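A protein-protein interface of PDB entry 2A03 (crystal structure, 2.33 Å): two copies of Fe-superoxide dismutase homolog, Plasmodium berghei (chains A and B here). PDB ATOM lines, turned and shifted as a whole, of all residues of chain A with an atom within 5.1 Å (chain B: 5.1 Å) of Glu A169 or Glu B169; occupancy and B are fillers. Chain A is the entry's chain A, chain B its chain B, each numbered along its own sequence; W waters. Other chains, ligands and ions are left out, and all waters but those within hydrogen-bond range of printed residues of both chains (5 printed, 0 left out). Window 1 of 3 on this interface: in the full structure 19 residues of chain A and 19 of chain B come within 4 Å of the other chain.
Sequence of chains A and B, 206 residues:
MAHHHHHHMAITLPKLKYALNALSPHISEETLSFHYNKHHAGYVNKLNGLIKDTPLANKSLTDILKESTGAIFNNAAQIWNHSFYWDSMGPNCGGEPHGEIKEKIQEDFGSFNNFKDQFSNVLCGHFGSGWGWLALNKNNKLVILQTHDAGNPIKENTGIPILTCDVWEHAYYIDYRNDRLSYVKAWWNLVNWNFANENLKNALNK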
ATOM      1  N   HIS A  39     -24.880  20.975  26.725  1.00  0.00           N
ATOM      2  CA  HIS A  39     -25.206  20.354  25.444  1.00  0.00           C
ATOM      3  C   HIS A  39     -25.593  18.867  25.575  1.00  0.00           C
ATOM      4  O   HIS A  39     -26.707  18.482  25.185  1.00  0.00           O
ATOM      5  CB  HIS A  39     -24.086  20.548  24.413  1.00  0.00           C
ATOM      6  CG  HIS A  39     -23.868  21.979  24.010  1.00  0.00           C
ATOM      7  ND1 HIS A  39     -24.649  22.620  23.076  1.00  0.00           N
ATOM      8  CD2 HIS A  39     -22.931  22.883  24.393  1.00  0.00           C
ATOM      9  CE1 HIS A  39     -24.220  23.859  22.917  1.00  0.00           C
ATOM     10  NE2 HIS A  39     -23.178  24.045  23.701  1.00  0.00           N
ATOM     11  N   SER A 129     -21.645  21.814  11.068  1.00  0.00           N
ATOM     12  CA  SER A 129     -21.614  20.949  12.238  1.00  0.00           C
ATOM     13  C   SER A 129     -21.424  19.506  11.818  1.00  0.00           C
ATOM     14  O   SER A 129     -21.945  19.066  10.801  1.00  0.00           O
ATOM     15  CB  SER A 129     -22.918  21.104  13.021  1.00  0.00           C
ATOM     16  OG  SER A 129     -23.127  22.469  13.363  1.00  0.00           O
ATOM     17  N   VAL A 167     -16.638  18.133  15.792  1.00  0.00           N
ATOM     18  CA  VAL A 167     -16.288  19.425  15.214  1.00  0.00           C
ATOM     19  C   VAL A 167     -17.460  20.418  15.106  1.00  0.00           C
ATOM     20  O   VAL A 167     -17.344  21.411  14.418  1.00  0.00           O
ATOM     21  CB  VAL A 167     -15.550  19.296  13.848  1.00  0.00           C
ATOM     22  CG1 VAL A 167     -14.249  18.465  14.006  1.00  0.00           C
ATOM     23  CG2 VAL A 167     -16.438  18.711  12.773  1.00  0.00           C
ATOM     24  N   TRP A 168     -18.567  20.188  15.815  1.00  0.00           N
ATOM     25  CA  TRP A 168     -19.509  21.308  16.087  1.00  0.00           C
ATOM     26  C   TRP A 168     -18.712  22.449  16.728  1.00  0.00           C
ATOM     27  O   TRP A 168     -17.834  22.200  17.571  1.00  0.00           O
ATOM     28  CB  TRP A 168     -20.626  20.904  17.051  1.00  0.00           C
ATOM     29  CG  TRP A 168     -21.678  20.006  16.455  1.00  0.00           C
ATOM     30  CD1 TRP A 168     -21.489  18.779  15.858  1.00  0.00           C
ATOM     31  CD2 TRP A 168     -23.087  20.254  16.407  1.00  0.00           C
ATOM     32  NE1 TRP A 168     -22.691  18.268  15.444  1.00  0.00           N
ATOM     33  CE2 TRP A 168     -23.686  19.149  15.768  1.00  0.00           C
ATOM     34  CE3 TRP A 168     -23.899  21.306  16.835  1.00  0.00           C
ATOM     35  CZ2 TRP A 168     -25.058  19.070  15.554  1.00  0.00           C
ATOM     36  CZ3 TRP A 168     -25.248  21.219  16.629  1.00  0.00           C
ATOM     37  CH2 TRP A 168     -25.819  20.112  15.992  1.00  0.00           C
ATOM     38  N   GLU A 169     -19.032  23.691  16.373  1.00  0.00           N
ATOM     39  CA  GLU A 169     -18.291  24.842  16.902  1.00  0.00           C
ATOM     40  C   GLU A 169     -18.241  24.867  18.447  1.00  0.00           C
ATOM     41  O   GLU A 169     -17.246  25.333  19.023  1.00  0.00           O
ATOM     42  CB  GLU A 169     -18.822  26.162  16.327  1.00  0.00           C
ATOM     43  CG  GLU A 169     -18.375  26.361  14.899  1.00  0.00           C
ATOM     44  CD  GLU A 169     -18.987  27.558  14.168  1.00  0.00           C
ATOM     45  OE1 GLU A 169     -20.164  27.927  14.412  1.00  0.00           O
ATOM     46  OE2 GLU A 169     -18.282  28.103  13.289  1.00  0.00           O
ATOM     47  N   HIS A 170     -19.284  24.363  19.108  1.00  0.00           N
ATOM     48  CA  HIS A 170     -19.361  24.396  20.583  1.00  0.00           C
ATOM     49  C   HIS A 170     -18.308  23.528  21.256  1.00  0.00           C
ATOM     50  O   HIS A 170     -18.015  23.701  22.445  1.00  0.00           O
ATOM     51  CB  HIS A 170     -20.774  24.016  21.101  1.00  0.00           C
ATOM     52  CG  HIS A 170     -21.182  22.591  20.847  1.00  0.00           C
ATOM     53  ND1 HIS A 170     -22.328  22.260  20.147  1.00  0.00           N
ATOM     54  CD2 HIS A 170     -20.635  21.414  21.247  1.00  0.00           C
ATOM     55  CE1 HIS A 170     -22.447  20.942  20.100  1.00  0.00           C
ATOM     56  NE2 HIS A 170     -21.429  20.405  20.754  1.00  0.00           N
ATOM     57  N   ALA A 171     -17.760  22.580  20.507  1.00  0.00           N
ATOM     58  CA  ALA A 171     -16.726  21.712  21.022  1.00  0.00           C
ATOM     59  C   ALA A 171     -15.440  22.483  21.269  1.00  0.00           C
ATOM     60  O   ALA A 171     -14.629  22.068  22.104  1.00  0.00           O
ATOM     61  CB  ALA A 171     -16.461  20.539  20.050  1.00  0.00           C
ATOM     62  N   TYR A 172     -15.253  23.602  20.558  1.00  0.00           N
ATOM     63  CA  TYR A 172     -13.976  24.329  20.618  1.00  0.00           C
ATOM     64  C   TYR A 172     -14.047  25.853  20.708  1.00  0.00           C
ATOM     65  O   TYR A 172     -13.039  26.494  20.957  1.00  0.00           O
ATOM     66  CB  TYR A 172     -13.094  23.919  19.427  1.00  0.00           C
ATOM     67  CG  TYR A 172     -13.651  24.249  18.049  1.00  0.00           C
ATOM     68  CD1 TYR A 172     -13.453  25.512  17.464  1.00  0.00           C
ATOM     69  CD2 TYR A 172     -14.353  23.288  17.316  1.00  0.00           C
ATOM     70  CE1 TYR A 172     -13.959  25.795  16.197  1.00  0.00           C
ATOM     71  CE2 TYR A 172     -14.854  23.560  16.067  1.00  0.00           C
ATOM     72  CZ  TYR A 172     -14.648  24.806  15.495  1.00  0.00           C
ATOM     73  OH  TYR A 172     -15.156  25.054  14.239  1.00  0.00           O
ATOM     74  N   TYR A 173     -15.218  26.447  20.531  1.00  0.00           N
ATOM     75  CA  TYR A 173     -15.289  27.894  20.435  1.00  0.00           C
ATOM     76  C   TYR A 173     -14.845  28.601  21.700  1.00  0.00           C
ATOM     77  O   TYR A 173     -14.265  29.684  21.631  1.00  0.00           O
ATOM     78  CB  TYR A 173     -16.692  28.386  20.018  1.00  0.00           C
ATOM     79  CG  TYR A 173     -16.554  29.554  19.076  1.00  0.00           C
ATOM     80  CD1 TYR A 173     -16.312  29.338  17.718  1.00  0.00           C
ATOM     81  CD2 TYR A 173     -16.562  30.866  19.553  1.00  0.00           C
ATOM     82  CE1 TYR A 173     -16.133  30.396  16.857  1.00  0.00           C
ATOM     83  CE2 TYR A 173     -16.382  31.931  18.700  1.00  0.00           C
ATOM     84  CZ  TYR A 173     -16.168  31.696  17.357  1.00  0.00           C
ATOM     85  OH  TYR A 173     -15.993  32.745  16.511  1.00  0.00           O
ATOM     86  N   HIS B  39     -14.249  35.158  10.751  1.00  0.00           N
ATOM     87  CA  HIS B  39     -15.154  34.319   9.965  1.00  0.00           C
ATOM     88  C   HIS B  39     -15.473  34.898   8.581  1.00  0.00           C
ATOM     89  O   HIS B  39     -15.176  34.275   7.555  1.00  0.00           O
ATOM     90  CB  HIS B  39     -16.452  34.029  10.735  1.00  0.00           C
ATOM     91  CG  HIS B  39     -16.250  33.140  11.929  1.00  0.00           C
ATOM     92  ND1 HIS B  39     -16.229  31.764  11.837  1.00  0.00           N
ATOM     93  CD2 HIS B  39     -16.005  33.437  13.228  1.00  0.00           C
ATOM     94  CE1 HIS B  39     -15.994  31.253  13.033  1.00  0.00           C
ATOM     95  NE2 HIS B  39     -15.855  32.247  13.896  1.00  0.00           N
ATOM     96  N   SER B 129     -25.864  24.021  12.087  1.00  0.00           N
ATOM     97  CA  SER B 129     -25.510  25.332  11.549  1.00  0.00           C
ATOM     98  C   SER B 129     -26.519  25.772  10.484  1.00  0.00           C
ATOM     99  O   SER B 129     -26.990  24.966   9.692  1.00  0.00           O
ATOM    100  CB  SER B 129     -24.107  25.286  10.933  1.00  0.00           C
ATOM    101  OG  SER B 129     -23.115  24.960  11.897  1.00  0.00           O
ATOM    102  N   VAL B 167     -27.629  31.553  12.781  1.00  0.00           N
ATOM    103  CA  VAL B 167     -27.688  30.733  13.988  1.00  0.00           C
ATOM    104  C   VAL B 167     -26.589  29.683  14.020  1.00  0.00           C
ATOM    105  O   VAL B 167     -26.676  28.700  14.747  1.00  0.00           O
ATOM    106  CB  VAL B 167     -29.098  30.128  14.265  1.00  0.00           C
ATOM    107  CG1 VAL B 167     -30.111  31.246  14.574  1.00  0.00           C
ATOM    108  CG2 VAL B 167     -29.586  29.241  13.100  1.00  0.00           C
ATOM    109  N   TRP B 168     -25.534  29.892  13.251  1.00  0.00           N
ATOM    110  CA  TRP B 168     -24.299  29.153  13.508  1.00  0.00           C
ATOM    111  C   TRP B 168     -23.860  29.502  14.945  1.00  0.00           C
ATOM    112  O   TRP B 168     -24.005  30.662  15.401  1.00  0.00           O
ATOM    113  CB  TRP B 168     -23.211  29.551  12.529  1.00  0.00           C
ATOM    114  CG  TRP B 168     -23.316  28.998  11.115  1.00  0.00           C
ATOM    115  CD1 TRP B 168     -24.336  29.199  10.205  1.00  0.00           C
ATOM    116  CD2 TRP B 168     -22.308  28.250  10.422  1.00  0.00           C
ATOM    117  NE1 TRP B 168     -24.035  28.566   9.006  1.00  0.00           N
ATOM    118  CE2 TRP B 168     -22.797  27.987   9.113  1.00  0.00           C
ATOM    119  CE3 TRP B 168     -21.043  27.758  10.787  1.00  0.00           C
ATOM    120  CZ2 TRP B 168     -22.063  27.259   8.175  1.00  0.00           C
ATOM    121  CZ3 TRP B 168     -20.318  27.031   9.858  1.00  0.00           C
ATOM    122  CH2 TRP B 168     -20.839  26.783   8.565  1.00  0.00           C
ATOM    123  N   GLU B 169     -23.339  28.516  15.664  1.00  0.00           N
ATOM    124  CA  GLU B 169     -22.925  28.721  17.072  1.00  0.00           C
ATOM    125  C   GLU B 169     -21.929  29.871  17.226  1.00  0.00           C
ATOM    126  O   GLU B 169     -21.960  30.604  18.216  1.00  0.00           O
ATOM    127  CB  GLU B 169     -22.398  27.412  17.692  1.00  0.00           C
ATOM    128  CG  GLU B 169     -23.528  26.439  17.949  1.00  0.00           C
ATOM    129  CD  GLU B 169     -23.099  25.037  18.351  1.00  0.00           C
ATOM    130  OE1 GLU B 169     -22.077  24.559  17.830  1.00  0.00           O
ATOM    131  OE2 GLU B 169     -23.823  24.399  19.170  1.00  0.00           O
ATOM    132  N   HIS B 170     -21.071  30.062  16.236  1.00  0.00           N
ATOM    133  CA  HIS B 170     -20.114  31.172  16.294  1.00  0.00           C
ATOM    134  C   HIS B 170     -20.778  32.549  16.300  1.00  0.00           C
ATOM    135  O   HIS B 170     -20.152  33.532  16.704  1.00  0.00           O
ATOM    136  CB  HIS B 170     -19.099  31.090  15.162  1.00  0.00           C
ATOM    137  CG  HIS B 170     -19.654  31.440  13.819  1.00  0.00           C
ATOM    138  ND1 HIS B 170     -19.586  30.581  12.746  1.00  0.00           N
ATOM    139  CD2 HIS B 170     -20.277  32.558  13.371  1.00  0.00           C
ATOM    140  CE1 HIS B 170     -20.156  31.150  11.696  1.00  0.00           C
ATOM    141  NE2 HIS B 170     -20.577  32.352  12.048  1.00  0.00           N
ATOM    142  N   ALA B 171     -22.032  32.641  15.861  1.00  0.00           N
ATOM    143  CA  ALA B 171     -22.746  33.920  15.934  1.00  0.00           C
ATOM    144  C   ALA B 171     -23.051  34.352  17.363  1.00  0.00           C
ATOM    145  O   ALA B 171     -23.204  35.560  17.608  1.00  0.00           O
ATOM    146  CB  ALA B 171     -24.018  33.909  15.108  1.00  0.00           C
ATOM    147  N   TYR B 172     -23.111  33.409  18.309  1.00  0.00           N
ATOM    148  CA  TYR B 172     -23.539  33.755  19.677  1.00  0.00           C
ATOM    149  C   TYR B 172     -22.750  33.135  20.812  1.00  0.00           C
ATOM    150  O   TYR B 172     -22.993  33.480  21.965  1.00  0.00           O
ATOM    151  CB  TYR B 172     -25.021  33.443  19.886  1.00  0.00           C
ATOM    152  CG  TYR B 172     -25.387  31.997  19.653  1.00  0.00           C
ATOM    153  CD1 TYR B 172     -25.271  31.053  20.669  1.00  0.00           C
ATOM    154  CD2 TYR B 172     -25.829  31.577  18.415  1.00  0.00           C
ATOM    155  CE1 TYR B 172     -25.589  29.718  20.445  1.00  0.00           C
ATOM    156  CE2 TYR B 172     -26.132  30.270  18.177  1.00  0.00           C
ATOM    157  CZ  TYR B 172     -26.039  29.343  19.200  1.00  0.00           C
ATOM    158  OH  TYR B 172     -26.362  28.035  18.942  1.00  0.00           O
ATOM    159  N   TYR B 173     -21.785  32.263  20.513  1.00  0.00           N
ATOM    160  CA  TYR B 173     -21.183  31.476  21.565  1.00  0.00           C
ATOM    161  C   TYR B 173     -20.367  32.349  22.512  1.00  0.00           C
ATOM    162  O   TYR B 173     -20.309  32.081  23.699  1.00  0.00           O
ATOM    163  CB  TYR B 173     -20.355  30.293  21.018  1.00  0.00           C
ATOM    164  CG  TYR B 173     -20.558  29.059  21.887  1.00  0.00           C
ATOM    165  CD1 TYR B 173     -21.719  28.304  21.769  1.00  0.00           C
ATOM    166  CD2 TYR B 173     -19.636  28.683  22.851  1.00  0.00           C
ATOM    167  CE1 TYR B 173     -21.952  27.220  22.559  1.00  0.00           C
ATOM    168  CE2 TYR B 173     -19.862  27.577  23.642  1.00  0.00           C
ATOM    169  CZ  TYR B 173     -21.047  26.857  23.495  1.00  0.00           C
ATOM    170  OH  TYR B 173     -21.321  25.760  24.272  1.00  0.00           O
HETATM  171  O   HOH W   1     -21.611  23.977  15.348  1.00  0.00           O
HETATM  172  O   HOH W   2     -24.558  21.998  10.327  1.00  0.00           O
HETATM  173  O   HOH W   3     -17.588  35.016  16.100  1.00  0.00           O
HETATM  174  O   HOH W   4     -19.529  23.677  24.950  1.00  0.00           O
HETATM  175  O   HOH W   5     -22.306  26.295  13.961  1.00  0.00           O
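Hydrophobic or aromatic side chains of chain B within 4 Å of the printed part of chain A: His B39, Trp B168, His B170 and Tyr B173. Among the printed residues, 12 pairs touch across the chains. Among the printed residues, no Asp or Glu carboxylate lies within 4 Å of a Lys or Arg side-chain nitrogen of the other chain.
NE2 of His A39 sits at hydrogen-bond distance from OH of Tyr B173. OG of Ser A129 is in hydrogen-bond range of OG of Ser B129. The side-chain carboxylate (OE1) of Glu A169 lies within hydrogen-bond range of the backbone NH (N) of Glu B169 (3.5 Å). The side-chain carboxylate (OE2) of Glu A169 sits at hydrogen-bond distance from a ring nitrogen (ND1) of His B170, at 2.9 Å. The side-chain carboxylate (OE2) of Glu B169 sits at hydrogen-bond distance from a ring nitrogen (ND1) of His A170 (2.8 Å). The side-chain hydroxyl (OH) of Tyr A173 is in hydrogen-bond range of a ring nitrogen (NE2) of His B39.
His A39 touches Tyr B173, and with the chains exchanged Tyr A173 touches His B39. Ser A129 touches its own counterpart, Ser B129. Glu B169 touches its own counterpart, Glu A169. His A170 touches Tyr B173, and with the chains exchanged Tyr A173 touches His B170.
Glu A169 touches just these residues of chain B: His B39 (3.9 Å), Trp B168 (3.7 Å), Glu B169 (3.5 Å) and His B170 (2.9 Å). Of chain A, only His A39 (3.8 Å), Trp A168 (3.9 Å), Glu A169 (3.5 Å) and His A170 (2.8 Å) come within 4 Å of Glu B169. Of the printed residues of chain B, Trp A168 touches Glu B169. Printed residues of chain B within 4 Å of His A39: Glu B169 and Tyr B173. Val B167 touches none of the printed residues of chain A. The nearest residue of chain A that does not touch Glu B169 is Ser A129 (5.0 Å).
Water W5 lies within hydrogen-bond range of the side-chain hydroxyl of Ser B129 (2.6 Å), the side-chain carboxylate of Glu A169 (2.7 Å) and the backbone NH of Glu B169 (3.0 Å). Water W1 lies within hydrogen-bond range of the side-chain carboxylate (OE1) of Glu B169 (2.6 Å), the backbone NH (N) of Glu A169 (2.8 Å) and the side-chain hydroxyl (OG) of Ser A129 (2.9 Å). Water W3 lies within hydrogen-bond range of OH of Tyr A173 (2.8 Å) and O of His B170 (3.0 Å). Water W4 bridges the side-chain hydroxyl of Tyr B173 and the backbone carbonyl oxygen of His A170. Water W2 lies within hydrogen-bond range of N of Ser B129 and N of Ser A129.
Among the printed residues, pairs that only touch across the chains: Tyr A173 with His B170 (3.5 Å), His A170 with Tyr B173 (3.7 Å), Glu A169 with Trp B168 (3.7 Å), His A39 with Glu B169 (3.8 Å), Trp A168 with Glu B169 (3.9 Å) and Glu A169 with His B39 (3.9 Å).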
